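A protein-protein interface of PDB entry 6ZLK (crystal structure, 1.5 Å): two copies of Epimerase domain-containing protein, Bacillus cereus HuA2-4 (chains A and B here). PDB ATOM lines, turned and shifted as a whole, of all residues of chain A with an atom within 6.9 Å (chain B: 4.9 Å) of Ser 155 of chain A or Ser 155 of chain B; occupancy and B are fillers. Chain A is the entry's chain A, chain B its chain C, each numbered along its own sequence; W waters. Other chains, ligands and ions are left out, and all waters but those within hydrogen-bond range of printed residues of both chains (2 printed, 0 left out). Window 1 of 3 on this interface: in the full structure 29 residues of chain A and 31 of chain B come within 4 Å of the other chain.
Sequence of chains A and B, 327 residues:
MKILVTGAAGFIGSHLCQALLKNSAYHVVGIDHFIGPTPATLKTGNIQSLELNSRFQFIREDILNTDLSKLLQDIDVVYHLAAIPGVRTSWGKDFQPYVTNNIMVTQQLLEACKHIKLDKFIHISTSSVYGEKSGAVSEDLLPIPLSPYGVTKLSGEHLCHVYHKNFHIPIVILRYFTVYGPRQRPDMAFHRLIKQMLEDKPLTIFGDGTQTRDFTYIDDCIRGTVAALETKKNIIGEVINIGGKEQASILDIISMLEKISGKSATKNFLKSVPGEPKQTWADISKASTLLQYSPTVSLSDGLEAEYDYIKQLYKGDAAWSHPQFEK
OG of Ser 155 of chain A sits close to OG of Ser 155 of chain B, 2.2 Å away.
Ile 103 of chain A touches its own counterpart, Ile 103 of chain B.
Val 151 of chain A touches Ser 155 of chain B, and with the chains exchanged Ser 155 of chain A touches Val 151 of chain B.
Val 151 of chain A touches His 158 of chain B, and with the chains exchanged His 158 of chain A touches Val 151 of chain B.
Leu 154 of chain A touches His 158 of chain B, and with the chains exchanged His 158 of chain A touches Leu 154 of chain B.
10 positions are printed for both chains.
Of the 8 pairs that touch across the chains among the printed residues, 8 have their exchanged pair printed and touching as well.
Water W2 lies within hydrogen-bond range of OG of Ser 155 of chain B (2.7 Å), ND1 of His 158 of chain A (2.8 Å), O of Val 151 of chain B (2.9 Å) and OG of Ser 155 of chain A (3.0 Å).
Water W1 lies within hydrogen-bond range of OG of Ser 155 of chain A (3.0 Å), O of Val 151 of chain A (3.0 Å), ND1 of His 158 of chain B (3.1 Å) and OG of Ser 155 of chain B (3.5 Å).
Ile 103 of chain A touches Ile 103 of chain B (CD1 to CD1, 3.6 Å).
Val 151 of chain A touches Ser 155 of chain B.
CB of His 158 of chain B touches CG2 of Val 151 of chain A (3.8 Å).
Leu 154 of chain A touches His 158 of chain B (CD2 to CE1, 3.3 Å).
O of Ser 155 of chain A touches CG1 of Val 151 of chain B (3.7 Å).
Val 151 of chain B touches His 158 of chain A.
His 158 of chain A touches Leu 154 of chain B (CE1 to CD2, 3.2 Å).
Of the printed residues of chain B, Ile 103 of chain A touches Ile 103 (3.6 Å).
Printed residues of chain B within 4 Å of Val 151 of chain A: Ser 155 (3.7 Å) and His 158 (3.8 Å).
Printed residues of chain B within 4 Å of Leu 154 of chain A: His 158 (3.3 Å).
Ser 155 of chain A touches just these residues of chain B: Val 151 (3.7 Å) and Ser 155 (2.2 Å).
Printed residues of chain B within 4 Å of His 158 of chain A: Val 151 (3.8 Å) and Leu 154 (3.2 Å).
Ser 155 of chain B touches just these residues of chain A: Val 151 and Ser 155.
Of the 10 printed residues of chain B, 5 touch a printed residue of chain A.
Of the 18 printed residues of chain A, 5 touch a printed residue of chain B.
Printed residues of chain A that touch a printed residue of chain B: Ile 103, Val 151, Leu 154, Ser 155 and His 158.
Hydrophobic or aromatic side chains of chain A within 4 Å of the printed part of chain B: Ile 103, Val 151, Leu 154 and His 158.
Among the printed residues, 8 pairs touch across the chains.
Among the printed residues, no Asp or Glu carboxylate lies within 4 Å of a Lys or Arg side-chain nitrogen of the other chain.
A ring nitrogen (ND1) of His 158 of chain A sits at hydrogen-bond distance from the backbone carbonyl oxygen of Leu 154 of chain A, at 3.4 Å.
The backbone carbonyl oxygen (O) of Val 151 of chain A is in hydrogen-bond range of the side-chain hydroxyl (OG) of Ser 155 of chain A (3.1 Å).
A ring nitrogen (ND1) of His 158 of chain B lies within hydrogen-bond range of the backbone carbonyl oxygen (O) of Leu 154 of chain B (3.4 Å).
The backbone carbonyl oxygen of Val 151 of chain B lies within hydrogen-bond range of the side-chain hydroxyl of Ser 155 of chain B.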
ATOM      1  N   ASN A 102      -0.737  28.081 -16.170  1.00  0.00           N
ATOM      2  CA  ASN A 102      -0.016  28.842 -15.141  1.00  0.00           C
ATOM      3  C   ASN A 102       0.569  27.879 -14.101  1.00  0.00           C
ATOM      4  O   ASN A 102       1.582  28.282 -13.462  1.00  0.00           O
ATOM      5  CB  ASN A 102      -0.860  29.912 -14.461  1.00  0.00           C
ATOM      6  CG  ASN A 102      -1.335  30.987 -15.428  1.00  0.00           C
ATOM      7  OD1 ASN A 102      -0.933  30.961 -16.605  1.00  0.00           O
ATOM      8  ND2 ASN A 102      -2.237  31.841 -14.994  1.00  0.00           N
ATOM      9  N   ILE A 103      -0.036  26.698 -13.891  1.00  0.00           N
ATOM     10  CA  ILE A 103       0.454  25.743 -12.862  1.00  0.00           C
ATOM     11  C   ILE A 103       1.135  24.546 -13.528  1.00  0.00           C
ATOM     12  O   ILE A 103       2.320  24.313 -13.262  1.00  0.00           O
ATOM     13  CB  ILE A 103      -0.674  25.319 -11.915  1.00  0.00           C
ATOM     14  CG1 ILE A 103      -1.398  26.524 -11.328  1.00  0.00           C
ATOM     15  CG2 ILE A 103      -0.114  24.437 -10.809  1.00  0.00           C
ATOM     16  CD1 ILE A 103      -2.484  26.216 -10.347  1.00  0.00           C
ATOM     17  N   THR A 106       4.355  25.410 -15.435  1.00  0.00           N
ATOM     18  CA  THR A 106       5.458  25.779 -14.540  1.00  0.00           C
ATOM     19  C   THR A 106       6.044  24.499 -13.932  1.00  0.00           C
ATOM     20  O   THR A 106       7.278  24.353 -13.909  1.00  0.00           O
ATOM     21  CB  THR A 106       4.992  26.761 -13.465  1.00  0.00           C
ATOM     22  OG1 THR A 106       4.544  27.978 -14.082  1.00  0.00           O
ATOM     23  CG2 THR A 106       6.085  27.124 -12.495  1.00  0.00           C
ATOM     24  N   HIS A 123      11.405  33.432 -13.020  1.00  0.00           N
ATOM     25  CA  HIS A 123       9.944  33.195 -13.071  1.00  0.00           C
ATOM     26  C   HIS A 123       9.214  34.504 -12.947  1.00  0.00           C
ATOM     27  O   HIS A 123       9.379  35.205 -11.932  1.00  0.00           O
ATOM     28  CB  HIS A 123       9.555  32.189 -11.988  1.00  0.00           C
ATOM     29  CG  HIS A 123       8.100  31.940 -11.955  1.00  0.00           C
ATOM     30  ND1 HIS A 123       7.539  30.935 -12.701  1.00  0.00           N
ATOM     31  CD2 HIS A 123       7.095  32.540 -11.278  1.00  0.00           C
ATOM     32  CE1 HIS A 123       6.226  30.959 -12.506  1.00  0.00           C
ATOM     33  NE2 HIS A 123       5.917  31.933 -11.629  1.00  0.00           N
ATOM     34  N   VAL A 129      -0.858  38.526  -6.874  1.00  0.00           N
ATOM     35  CA  VAL A 129      -0.758  37.536  -5.768  1.00  0.00           C
ATOM     36  C   VAL A 129      -1.066  38.221  -4.442  1.00  0.00           C
ATOM     37  O   VAL A 129      -1.459  37.500  -3.505  1.00  0.00           O
ATOM     38  CB  VAL A 129       0.603  36.826  -5.699  1.00  0.00           C
ATOM     39  CG1 VAL A 129       0.952  36.098  -7.004  1.00  0.00           C
ATOM     40  CG2 VAL A 129       1.715  37.725  -5.222  1.00  0.00           C
ATOM     41  N   TYR A 149      -7.077  34.086 -11.175  1.00  0.00           N
ATOM     42  CA  TYR A 149      -5.785  34.357 -11.863  1.00  0.00           C
ATOM     43  C   TYR A 149      -4.642  34.440 -10.850  1.00  0.00           C
ATOM     44  O   TYR A 149      -3.610  33.777 -11.001  1.00  0.00           O
ATOM     45  CB  TYR A 149      -5.896  35.670 -12.646  1.00  0.00           C
ATOM     46  CG  TYR A 149      -4.582  36.222 -13.109  1.00  0.00           C
ATOM     47  CD1 TYR A 149      -3.722  35.509 -13.936  1.00  0.00           C
ATOM     48  CD2 TYR A 149      -4.156  37.469 -12.683  1.00  0.00           C
ATOM     49  CE1 TYR A 149      -2.529  36.035 -14.398  1.00  0.00           C
ATOM     50  CE2 TYR A 149      -2.932  37.976 -13.078  1.00  0.00           C
ATOM     51  CZ  TYR A 149      -2.117  37.267 -13.942  1.00  0.00           C
ATOM     52  OH  TYR A 149      -0.941  37.763 -14.397  1.00  0.00           O
ATOM     53  N   GLY A 150      -4.807  35.281  -9.836  1.00  0.00           N
ATOM     54  CA  GLY A 150      -3.785  35.543  -8.835  1.00  0.00           C
ATOM     55  C   GLY A 150      -3.469  34.266  -8.104  1.00  0.00           C
ATOM     56  O   GLY A 150      -2.310  34.031  -7.795  1.00  0.00           O
ATOM     57  N   VAL A 151      -4.510  33.478  -7.837  1.00  0.00           N
ATOM     58  CA  VAL A 151      -4.260  32.185  -7.168  1.00  0.00           C
ATOM     59  C   VAL A 151      -3.309  31.343  -8.032  1.00  0.00           C
ATOM     60  O   VAL A 151      -2.370  30.715  -7.511  1.00  0.00           O
ATOM     61  CB  VAL A 151      -5.567  31.438  -6.887  1.00  0.00           C
ATOM     62  CG1 VAL A 151      -5.212  30.088  -6.314  1.00  0.00           C
ATOM     63  CG2 VAL A 151      -6.458  32.239  -5.952  1.00  0.00           C
ATOM     64  N   THR A 152      -3.591  31.183  -9.312  1.00  0.00           N
ATOM     65  CA  THR A 152      -2.776  30.309 -10.158  1.00  0.00           C
ATOM     66  C   THR A 152      -1.334  30.821 -10.283  1.00  0.00           C
ATOM     67  O   THR A 152      -0.410  30.001 -10.348  1.00  0.00           O
ATOM     68  CB  THR A 152      -3.378  30.108 -11.547  1.00  0.00           C
ATOM     69  OG1 THR A 152      -3.380  31.329 -12.299  1.00  0.00           O
ATOM     70  CG2 THR A 152      -4.763  29.514 -11.461  1.00  0.00           C
ATOM     71  N   LYS A 153      -1.136  32.137 -10.314  1.00  0.00           N
ATOM     72  CA  LYS A 153       0.216  32.728 -10.391  1.00  0.00           C
ATOM     73  C   LYS A 153       0.944  32.472  -9.060  1.00  0.00           C
ATOM     74  O   LYS A 153       2.129  32.101  -9.093  1.00  0.00           O
ATOM     75  CB  LYS A 153       0.098  34.206 -10.755  1.00  0.00           C
ATOM     76  CG  LYS A 153      -0.407  34.428 -12.188  1.00  0.00           C
ATOM     77  CD  LYS A 153       0.495  33.982 -13.271  1.00  0.00           C
ATOM     78  CE  LYS A 153       1.836  34.705 -13.221  1.00  0.00           C
ATOM     79  NZ  LYS A 153       2.724  34.456 -14.389  1.00  0.00           N
ATOM     80  N   LEU A 154       0.221  32.605  -7.956  1.00  0.00           N
ATOM     81  CA  LEU A 154       0.848  32.325  -6.647  1.00  0.00           C
ATOM     82  C   LEU A 154       1.233  30.839  -6.593  1.00  0.00           C
ATOM     83  O   LEU A 154       2.306  30.546  -6.084  1.00  0.00           O
ATOM     84  CB  LEU A 154      -0.077  32.741  -5.518  1.00  0.00           C
ATOM     85  CG  LEU A 154       0.489  32.521  -4.112  1.00  0.00           C
ATOM     86  CD1 LEU A 154       1.832  33.202  -3.925  1.00  0.00           C
ATOM     87  CD2 LEU A 154      -0.540  32.987  -3.085  1.00  0.00           C
ATOM     88  N   SER A 155       0.405  29.927  -7.086  1.00  0.00           N
ATOM     89  CA  SER A 155       0.783  28.478  -7.116  1.00  0.00           C
ATOM     90  C   SER A 155       2.052  28.279  -7.947  1.00  0.00           C
ATOM     91  O   SER A 155       2.946  27.488  -7.600  1.00  0.00           O
ATOM     92  CB  SER A 155      -0.296  27.617  -7.630  1.00  0.00           C
ATOM     93  OG  SER A 155      -1.439  27.790  -6.814  1.00  0.00           O
ATOM     94  N   GLY A 156       2.213  29.044  -9.030  1.00  0.00           N
ATOM     95  CA  GLY A 156       3.454  28.977  -9.812  1.00  0.00           C
ATOM     96  C   GLY A 156       4.663  29.397  -9.002  1.00  0.00           C
ATOM     97  O   GLY A 156       5.677  28.709  -9.067  1.00  0.00           O
ATOM     98  N   GLU A 157       4.559  30.422  -8.175  1.00  0.00           N
ATOM     99  CA  GLU A 157       5.678  30.879  -7.331  1.00  0.00           C
ATOM    100  C   GLU A 157       5.955  29.761  -6.331  1.00  0.00           C
ATOM    101  O   GLU A 157       7.089  29.441  -6.097  1.00  0.00           O
ATOM    102  CB  GLU A 157       5.361  32.115  -6.505  1.00  0.00           C
ATOM    103  CG  GLU A 157       5.061  33.346  -7.317  1.00  0.00           C
ATOM    104  CD  GLU A 157       5.002  34.578  -6.439  1.00  0.00           C
ATOM    105  OE1 GLU A 157       5.361  34.476  -5.243  1.00  0.00           O
ATOM    106  OE2 GLU A 157       4.599  35.645  -6.935  1.00  0.00           O
ATOM    107  N   HIS A 158       4.904  29.168  -5.770  1.00  0.00           N
ATOM    108  CA  HIS A 158       5.113  28.121  -4.738  1.00  0.00           C
ATOM    109  C   HIS A 158       5.844  26.951  -5.389  1.00  0.00           C
ATOM    110  O   HIS A 158       6.721  26.331  -4.734  1.00  0.00           O
ATOM    111  CB  HIS A 158       3.760  27.706  -4.122  1.00  0.00           C
ATOM    112  CG  HIS A 158       3.152  28.756  -3.235  1.00  0.00           C
ATOM    113  ND1 HIS A 158       1.799  28.885  -3.117  1.00  0.00           N
ATOM    114  CD2 HIS A 158       3.689  29.657  -2.415  1.00  0.00           C
ATOM    115  CE1 HIS A 158       1.536  29.808  -2.225  1.00  0.00           C
ATOM    116  NE2 HIS A 158       2.665  30.317  -1.796  1.00  0.00           N
ATOM    117  N   LEU A 159       5.473  26.542  -6.603  1.00  0.00           N
ATOM    118  CA  LEU A 159       6.187  25.455  -7.283  1.00  0.00           C
ATOM    119  C   LEU A 159       7.673  25.799  -7.421  1.00  0.00           C
ATOM    120  O   LEU A 159       8.535  24.957  -7.166  1.00  0.00           O
ATOM    121  CB  LEU A 159       5.577  25.218  -8.667  1.00  0.00           C
ATOM    122  CG  LEU A 159       4.264  24.453  -8.643  1.00  0.00           C
ATOM    123  CD1 LEU A 159       3.628  24.478 -10.028  1.00  0.00           C
ATOM    124  CD2 LEU A 159       4.482  23.034  -8.158  1.00  0.00           C
ATOM    125  N   CYS A 160       8.005  27.029  -7.795  1.00  0.00           N
ATOM    126  CA  CYS A 160       9.415  27.464  -7.852  1.00  0.00           C
ATOM    127  C   CYS A 160      10.086  27.213  -6.491  1.00  0.00           C
ATOM    128  O   CYS A 160      11.173  26.611  -6.502  1.00  0.00           O
ATOM    129  CB  CYS A 160       9.576  28.929  -8.236  1.00  0.00           C
ATOM    130  SG  CYS A 160       9.118  29.273  -9.961  1.00  0.00           S
ATOM    131  N   HIS A 161       9.451  27.599  -5.380  1.00  0.00           N
ATOM    132  CA  HIS A 161      10.108  27.371  -4.078  1.00  0.00           C
ATOM    133  C   HIS A 161      10.239  25.870  -3.824  1.00  0.00           C
ATOM    134  O   HIS A 161      11.255  25.478  -3.215  1.00  0.00           O
ATOM    135  CB  HIS A 161       9.346  28.035  -2.957  1.00  0.00           C
ATOM    136  CG  HIS A 161       9.390  29.517  -3.046  1.00  0.00           C
ATOM    137  ND1 HIS A 161      10.603  30.210  -2.951  1.00  0.00           N
ATOM    138  CD2 HIS A 161       8.415  30.433  -3.183  1.00  0.00           C
ATOM    139  CE1 HIS A 161      10.335  31.510  -3.060  1.00  0.00           C
ATOM    140  NE2 HIS A 161       9.011  31.665  -3.168  1.00  0.00           N
ATOM    141  N   ILE B 103      -7.498  21.482  -7.121  1.00  0.00           N
ATOM    142  CA  ILE B 103      -7.713  22.905  -7.520  1.00  0.00           C
ATOM    143  C   ILE B 103      -8.998  23.036  -8.345  1.00  0.00           C
ATOM    144  O   ILE B 103      -9.853  23.734  -7.902  1.00  0.00           O
ATOM    145  CB  ILE B 103      -6.470  23.496  -8.223  1.00  0.00           C
ATOM    146  CG1 ILE B 103      -5.180  23.211  -7.447  1.00  0.00           C
ATOM    147  CG2 ILE B 103      -6.685  24.962  -8.539  1.00  0.00           C
ATOM    148  CD1 ILE B 103      -3.929  23.773  -8.078  1.00  0.00           C
ATOM    149  N   VAL B 151       1.391  22.556  -2.421  1.00  0.00           N
ATOM    150  CA  VAL B 151       1.047  23.695  -3.305  1.00  0.00           C
ATOM    151  C   VAL B 151      -0.414  23.610  -3.700  1.00  0.00           C
ATOM    152  O   VAL B 151      -1.125  24.661  -3.711  1.00  0.00           O
ATOM    153  CB  VAL B 151       1.967  23.714  -4.531  1.00  0.00           C
ATOM    154  CG1 VAL B 151       1.484  24.772  -5.532  1.00  0.00           C
ATOM    155  CG2 VAL B 151       3.394  23.965  -4.093  1.00  0.00           C
ATOM    156  N   THR B 152      -0.861  22.432  -4.135  1.00  0.00           N
ATOM    157  CA  THR B 152      -2.228  22.295  -4.668  1.00  0.00           C
ATOM    158  C   THR B 152      -3.241  22.529  -3.542  1.00  0.00           C
ATOM    159  O   THR B 152      -4.264  23.136  -3.791  1.00  0.00           O
ATOM    160  CB  THR B 152      -2.459  21.000  -5.436  1.00  0.00           C
ATOM    161  OG1 THR B 152      -2.384  19.885  -4.530  1.00  0.00           O
ATOM    162  CG2 THR B 152      -1.454  20.840  -6.543  1.00  0.00           C
ATOM    163  N   LYS B 153      -2.968  22.056  -2.328  1.00  0.00           N
ATOM    164  CA  LYS B 153      -3.905  22.271  -1.209  1.00  0.00           C
ATOM    165  C   LYS B 153      -3.930  23.768  -0.824  1.00  0.00           C
ATOM    166  O   LYS B 153      -5.010  24.295  -0.555  1.00  0.00           O
ATOM    167  CB  LYS B 153      -3.479  21.332  -0.079  1.00  0.00           C
ATOM    168  CG  LYS B 153      -3.695  19.856  -0.382  1.00  0.00           C
ATOM    169  CD  LYS B 153      -5.161  19.435  -0.467  1.00  0.00           C
ATOM    170  CE  LYS B 153      -5.977  19.756   0.774  1.00  0.00           C
ATOM    171  NZ  LYS B 153      -7.329  19.127   0.722  1.00  0.00           N
ATOM    172  N   LEU B 154      -2.781  24.451  -0.871  1.00  0.00           N
ATOM    173  CA  LEU B 154      -2.750  25.885  -0.541  1.00  0.00           C
ATOM    174  C   LEU B 154      -3.503  26.634  -1.643  1.00  0.00           C
ATOM    175  O   LEU B 154      -4.214  27.524  -1.304  1.00  0.00           O
ATOM    176  CB  LEU B 154      -1.304  26.317  -0.402  1.00  0.00           C
ATOM    177  CG  LEU B 154      -1.105  27.767  -0.016  1.00  0.00           C
ATOM    178  CD1 LEU B 154      -1.858  28.161   1.235  1.00  0.00           C
ATOM    179  CD2 LEU B 154       0.362  28.037   0.167  1.00  0.00           C
ATOM    180  N   SER B 155      -3.418  26.176  -2.883  1.00  0.00           N
ATOM    181  CA  SER B 155      -4.192  26.817  -3.989  1.00  0.00           C
ATOM    182  C   SER B 155      -5.688  26.688  -3.714  1.00  0.00           C
ATOM    183  O   SER B 155      -6.435  27.650  -3.838  1.00  0.00           O
ATOM    184  CB  SER B 155      -3.851  26.166  -5.282  1.00  0.00           C
ATOM    185  OG  SER B 155      -2.474  26.348  -5.513  1.00  0.00           O
ATOM    186  N   GLY B 156      -6.128  25.542  -3.203  1.00  0.00           N
ATOM    187  CA  GLY B 156      -7.552  25.376  -2.872  1.00  0.00           C
ATOM    188  C   GLY B 156      -7.959  26.319  -1.749  1.00  0.00           C
ATOM    189  O   GLY B 156      -9.055  26.919  -1.804  1.00  0.00           O
ATOM    190  N   GLU B 157      -7.117  26.466  -0.720  1.00  0.00           N
ATOM    191  CA  GLU B 157      -7.380  27.440   0.369  1.00  0.00           C
ATOM    192  C   GLU B 157      -7.560  28.831  -0.250  1.00  0.00           C
ATOM    193  O   GLU B 157      -8.459  29.569   0.154  1.00  0.00           O
ATOM    194  CB  GLU B 157      -6.265  27.569   1.396  1.00  0.00           C
ATOM    195  CG  GLU B 157      -6.050  26.325   2.229  1.00  0.00           C
ATOM    196  CD  GLU B 157      -5.160  26.581   3.425  1.00  0.00           C
ATOM    197  OE1 GLU B 157      -4.979  27.730   3.818  1.00  0.00           O
ATOM    198  OE2 GLU B 157      -4.687  25.602   4.044  1.00  0.00           O
ATOM    199  N   HIS B 158      -6.595  29.225  -1.108  1.00  0.00           N
ATOM    200  CA  HIS B 158      -6.651  30.580  -1.708  1.00  0.00           C
ATOM    201  C   HIS B 158      -7.935  30.717  -2.531  1.00  0.00           C
ATOM    202  O   HIS B 158      -8.513  31.843  -2.510  1.00  0.00           O
ATOM    203  CB  HIS B 158      -5.391  30.855  -2.529  1.00  0.00           C
ATOM    204  CG  HIS B 158      -4.238  31.137  -1.627  1.00  0.00           C
ATOM    205  ND1 HIS B 158      -2.978  30.663  -1.867  1.00  0.00           N
ATOM    206  CD2 HIS B 158      -4.113  31.948  -0.568  1.00  0.00           C
ATOM    207  CE1 HIS B 158      -2.178  31.089  -0.904  1.00  0.00           C
ATOM    208  NE2 HIS B 158      -2.815  31.822  -0.123  1.00  0.00           N
ATOM    209  N   LEU B 159      -8.375  29.701  -3.267  1.00  0.00           N
ATOM    210  CA  LEU B 159      -9.692  29.809  -3.942  1.00  0.00           C
ATOM    211  C   LEU B 159     -10.795  30.101  -2.926  1.00  0.00           C
ATOM    212  O   LEU B 159     -11.672  30.908  -3.204  1.00  0.00           O
ATOM    213  CB  LEU B 159     -10.006  28.571  -4.770  1.00  0.00           C
ATOM    214  CG  LEU B 159      -9.145  28.416  -6.013  1.00  0.00           C
ATOM    215  CD1 LEU B 159      -9.210  27.008  -6.528  1.00  0.00           C
ATOM    216  CD2 LEU B 159      -9.589  29.444  -7.068  1.00  0.00           C
HETATM  217  O   HOH W   1      -2.217  29.686  -4.671  1.00  0.00           O
HETATM  218  O   HOH W   2      -0.479  27.433  -4.005  1.00  0.00           O
